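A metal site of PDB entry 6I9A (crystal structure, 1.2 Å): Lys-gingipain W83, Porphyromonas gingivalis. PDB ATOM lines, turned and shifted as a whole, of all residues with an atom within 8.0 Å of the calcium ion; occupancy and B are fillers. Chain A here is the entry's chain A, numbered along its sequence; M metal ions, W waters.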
ATOM      1  N   HIS A   6     -12.948  -1.310  14.732  1.00  0.00           N
ATOM      2  CA  HIS A   6     -13.996  -1.285  13.734  1.00  0.00           C
ATOM      3  C   HIS A   6     -14.116   0.042  13.089  1.00  0.00           C
ATOM      4  O   HIS A   6     -15.161   0.721  13.219  1.00  0.00           O
ATOM      5  CB  HIS A   6     -15.336  -1.663  14.381  1.00  0.00           C
ATOM      6  CG  HIS A   6     -15.374  -3.071  14.845  1.00  0.00           C
ATOM      7  ND1 HIS A   6     -15.348  -4.120  13.959  1.00  0.00           N
ATOM      8  CD2 HIS A   6     -15.459  -3.546  16.090  1.00  0.00           C
ATOM      9  CE1 HIS A   6     -15.405  -5.224  14.714  1.00  0.00           C
ATOM     10  NE2 HIS A   6     -15.434  -4.908  16.009  1.00  0.00           N
ATOM     11  N   TYR A  67     -20.078 -12.332   0.640  1.00  0.00           N
ATOM     12  CA  TYR A  67     -19.065 -11.634   1.418  1.00  0.00           C
ATOM     13  C   TYR A  67     -17.881 -12.567   1.684  1.00  0.00           C
ATOM     14  O   TYR A  67     -16.729 -12.167   1.515  1.00  0.00           O
ATOM     15  CB  TYR A  67     -19.690 -11.144   2.744  1.00  0.00           C
ATOM     16  CG  TYR A  67     -18.620 -10.484   3.567  1.00  0.00           C
ATOM     17  CD1 TYR A  67     -17.918 -11.209   4.520  1.00  0.00           C
ATOM     18  CD2 TYR A  67     -18.232  -9.154   3.327  1.00  0.00           C
ATOM     19  CE1 TYR A  67     -16.817 -10.665   5.167  1.00  0.00           C
ATOM     20  CE2 TYR A  67     -17.122  -8.600   3.962  1.00  0.00           C
ATOM     21  CZ  TYR A  67     -16.428  -9.348   4.898  1.00  0.00           C
ATOM     22  OH  TYR A  67     -15.354  -8.805   5.568  1.00  0.00           O
ATOM     23  N   LEU A 103     -29.726  -5.501   9.886  1.00  0.00           N
ATOM     24  CA  LEU A 103     -28.375  -5.781  10.387  1.00  0.00           C
ATOM     25  C   LEU A 103     -27.883  -7.157   9.999  1.00  0.00           C
ATOM     26  O   LEU A 103     -26.664  -7.303   9.687  1.00  0.00           O
ATOM     27  CB  LEU A 103     -28.361  -5.674  11.929  1.00  0.00           C
ATOM     28  CG  LEU A 103     -26.987  -5.971  12.576  1.00  0.00           C
ATOM     29  CD1 LEU A 103     -25.897  -5.013  12.138  1.00  0.00           C
ATOM     30  CD2 LEU A 103     -27.108  -5.986  14.081  1.00  0.00           C
ATOM     31  N   SER A 106     -25.961  -7.846   6.849  1.00  0.00           N
ATOM     32  CA  SER A 106     -24.603  -7.244   6.876  1.00  0.00           C
ATOM     33  C   SER A 106     -23.665  -7.914   7.882  1.00  0.00           C
ATOM     34  O   SER A 106     -22.452  -7.856   7.683  1.00  0.00           O
ATOM     35  CB  SER A 106     -24.695  -5.743   7.191  1.00  0.00           C
ATOM     36  OG  SER A 106     -24.982  -5.396   8.533  1.00  0.00           O
ATOM     37  N   ALA A 107     -24.195  -8.507   8.925  1.00  0.00           N
ATOM     38  CA  ALA A 107     -23.413  -9.074  10.017  1.00  0.00           C
ATOM     39  C   ALA A 107     -23.177 -10.505   9.670  1.00  0.00           C
ATOM     40  O   ALA A 107     -24.062 -11.346   9.841  1.00  0.00           O
ATOM     41  CB  ALA A 107     -24.170  -8.900  11.343  1.00  0.00           C
ATOM     42  N   VAL A 108     -21.979 -10.788   9.157  1.00  0.00           N
ATOM     43  CA  VAL A 108     -21.701 -12.117   8.584  1.00  0.00           C
ATOM     44  C   VAL A 108     -21.051 -13.057   9.605  1.00  0.00           C
ATOM     45  O   VAL A 108     -21.471 -14.220   9.750  1.00  0.00           O
ATOM     46  CB  VAL A 108     -20.847 -11.998   7.318  1.00  0.00           C
ATOM     47  CG1 VAL A 108     -20.575 -13.368   6.711  1.00  0.00           C
ATOM     48  CG2 VAL A 108     -21.508 -11.084   6.302  1.00  0.00           C
ATOM     49  N   ASP A 109     -20.041 -12.572  10.335  1.00  0.00           N
ATOM     50  CA  ASP A 109     -19.404 -13.376  11.354  1.00  0.00           C
ATOM     51  C   ASP A 109     -20.228 -13.242  12.656  1.00  0.00           C
ATOM     52  O   ASP A 109     -21.379 -12.754  12.625  1.00  0.00           O
ATOM     53  CB  ASP A 109     -17.900 -13.079  11.506  1.00  0.00           C
ATOM     54  CG  ASP A 109     -17.513 -11.645  11.746  1.00  0.00           C
ATOM     55  OD1 ASP A 109     -18.286 -10.912  12.331  1.00  0.00           O
ATOM     56  OD2 ASP A 109     -16.408 -11.277  11.346  1.00  0.00           O
ATOM     57  N   GLY A 110     -19.741 -13.782  13.771  1.00  0.00           N
ATOM     58  CA  GLY A 110     -20.575 -13.946  14.948  1.00  0.00           C
ATOM     59  C   GLY A 110     -21.011 -12.736  15.740  1.00  0.00           C
ATOM     60  O   GLY A 110     -21.886 -12.863  16.601  1.00  0.00           O
ATOM     61  N   ASP A 111     -20.342 -11.602  15.533  1.00  0.00           N
ATOM     62  CA  ASP A 111     -20.642 -10.465  16.400  1.00  0.00           C
ATOM     63  C   ASP A 111     -21.767  -9.608  15.790  1.00  0.00           C
ATOM     64  O   ASP A 111     -22.408  -9.979  14.788  1.00  0.00           O
ATOM     65  CB  ASP A 111     -19.356  -9.709  16.697  1.00  0.00           C
ATOM     66  CG  ASP A 111     -18.774  -8.969  15.541  1.00  0.00           C
ATOM     67  OD1 ASP A 111     -19.491  -8.822  14.478  1.00  0.00           O
ATOM     68  OD2 ASP A 111     -17.627  -8.501  15.650  1.00  0.00           O
ATOM     69  N   TYR A 112     -21.997  -8.429  16.403  1.00  0.00           N
ATOM     70  CA  TYR A 112     -23.090  -7.586  15.887  1.00  0.00           C
ATOM     71  C   TYR A 112     -22.597  -6.413  15.034  1.00  0.00           C
ATOM     72  O   TYR A 112     -23.388  -5.520  14.652  1.00  0.00           O
ATOM     73  CB  TYR A 112     -24.033  -7.103  17.005  1.00  0.00           C
ATOM     74  CG  TYR A 112     -23.350  -6.424  18.174  1.00  0.00           C
ATOM     75  CD1 TYR A 112     -22.638  -5.233  17.999  1.00  0.00           C
ATOM     76  CD2 TYR A 112     -23.399  -6.978  19.445  1.00  0.00           C
ATOM     77  CE1 TYR A 112     -21.982  -4.613  19.065  1.00  0.00           C
ATOM     78  CE2 TYR A 112     -22.782  -6.349  20.515  1.00  0.00           C
ATOM     79  CZ  TYR A 112     -22.064  -5.164  20.322  1.00  0.00           C
ATOM     80  OH  TYR A 112     -21.432  -4.530  21.363  1.00  0.00           O
ATOM     81  N   PHE A 113     -21.294  -6.391  14.725  1.00  0.00           N
ATOM     82  CA  PHE A 113     -20.758  -5.377  13.846  1.00  0.00           C
ATOM     83  C   PHE A 113     -20.882  -5.772  12.394  1.00  0.00           C
ATOM     84  O   PHE A 113     -20.429  -6.885  12.024  1.00  0.00           O
ATOM     85  CB  PHE A 113     -19.290  -5.091  14.133  1.00  0.00           C
ATOM     86  CG  PHE A 113     -19.033  -4.465  15.478  1.00  0.00           C
ATOM     87  CD1 PHE A 113     -19.114  -3.092  15.634  1.00  0.00           C
ATOM     88  CD2 PHE A 113     -18.739  -5.247  16.581  1.00  0.00           C
ATOM     89  CE1 PHE A 113     -18.845  -2.494  16.881  1.00  0.00           C
ATOM     90  CE2 PHE A 113     -18.478  -4.653  17.826  1.00  0.00           C
ATOM     91  CZ  PHE A 113     -18.544  -3.280  17.966  1.00  0.00           C
ATOM     92  N   PRO A 114     -21.455  -4.943  11.548  1.00  0.00           N
ATOM     93  CA  PRO A 114     -21.532  -5.284  10.119  1.00  0.00           C
ATOM     94  C   PRO A 114     -20.188  -5.499   9.464  1.00  0.00           C
ATOM     95  O   PRO A 114     -19.198  -4.835   9.810  1.00  0.00           O
ATOM     96  CB  PRO A 114     -22.196  -4.043   9.481  1.00  0.00           C
ATOM     97  CG  PRO A 114     -22.946  -3.416  10.629  1.00  0.00           C
ATOM     98  CD  PRO A 114     -22.064  -3.629  11.832  1.00  0.00           C
ATOM     99  N   GLU A 115     -20.185  -6.355   8.432  1.00  0.00           N
ATOM    100  CA  GLU A 115     -19.027  -6.545   7.520  1.00  0.00           C
ATOM    101  C   GLU A 115     -19.062  -5.614   6.348  1.00  0.00           C
ATOM    102  O   GLU A 115     -18.033  -5.471   5.687  1.00  0.00           O
ATOM    103  CB  GLU A 115     -19.003  -8.016   7.026  1.00  0.00           C
ATOM    104  CG  GLU A 115     -18.142  -8.911   7.925  1.00  0.00           C
ATOM    105  CD  GLU A 115     -18.535  -8.873   9.387  1.00  0.00           C
ATOM    106  OE1 GLU A 115     -17.831  -8.200  10.166  1.00  0.00           O
ATOM    107  OE2 GLU A 115     -19.575  -9.484   9.762  1.00  0.00           O
ATOM    108  N   MET A 116     -20.244  -5.035   6.033  1.00  0.00           N
ATOM    109  CA  MET A 116     -20.462  -4.199   4.875  1.00  0.00           C
ATOM    110  C   MET A 116     -21.295  -2.994   5.284  1.00  0.00           C
ATOM    111  O   MET A 116     -22.198  -3.144   6.119  1.00  0.00           O
ATOM    112  CB  MET A 116     -21.222  -4.965   3.792  1.00  0.00           C
ATOM    113  CG  MET A 116     -20.410  -6.109   3.179  1.00  0.00           C
ATOM    114  SD  MET A 116     -21.442  -7.298   2.252  1.00  0.00           S
ATOM    115  CE  MET A 116     -22.195  -8.204   3.638  1.00  0.00           C
ATOM    116  N   TRP A 330     -22.328   4.800  11.064  1.00  0.00           N
ATOM    117  CA  TRP A 330     -21.336   3.898  11.648  1.00  0.00           C
ATOM    118  C   TRP A 330     -20.652   4.598  12.811  1.00  0.00           C
ATOM    119  O   TRP A 330     -20.515   4.053  13.906  1.00  0.00           O
ATOM    120  CB  TRP A 330     -20.319   3.545  10.564  1.00  0.00           C
ATOM    121  CG  TRP A 330     -19.336   2.503  11.008  1.00  0.00           C
ATOM    122  CD1 TRP A 330     -18.148   2.719  11.632  1.00  0.00           C
ATOM    123  CD2 TRP A 330     -19.445   1.108  10.775  1.00  0.00           C
ATOM    124  NE1 TRP A 330     -17.508   1.490  11.834  1.00  0.00           N
ATOM    125  CE2 TRP A 330     -18.284   0.500  11.302  1.00  0.00           C
ATOM    126  CE3 TRP A 330     -20.413   0.312  10.177  1.00  0.00           C
ATOM    127  CZ2 TRP A 330     -18.085  -0.897  11.242  1.00  0.00           C
ATOM    128  CZ3 TRP A 330     -20.214  -1.039  10.114  1.00  0.00           C
ATOM    129  CH2 TRP A 330     -19.076  -1.629  10.649  1.00  0.00           C
HETATM  130 CA    CA M   1     -19.165  -8.799  12.138  1.00  0.00          CA
HETATM  131  O   HOH W   1     -21.241 -10.039  12.339  1.00  0.00           O
HETATM  132  O   HOH W   2     -17.229  -7.753  13.075  1.00  0.00           O
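The nearest printed residue that does not touch the calcium ion is Pro 114 (4.4 Å).
The side-chain carboxylate of Glu 115 lies close to the backbone NH of Val 108, at 2.8 Å.
N of Glu 115 is in hydrogen-bond range of O of Ser 106, 2.8 Å away.
The calcium ion is bound by the side-chain carboxylate (OD1) of Asp 109 (2.3 Å), the backbone carbonyl oxygen (O) of Phe 113 (2.3 Å), the side-chain carboxylate (OD1) of Asp 111 (2.4 Å), water W2 (2.4 Å), water W1 (2.4 Å), the side-chain carboxylate (OE1) of Glu 115 (2.5 Å) and the side-chain carboxylate (OE2) of Glu 115 (2.5 Å).
The calcium ion has seven donor atoms within binding distance.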
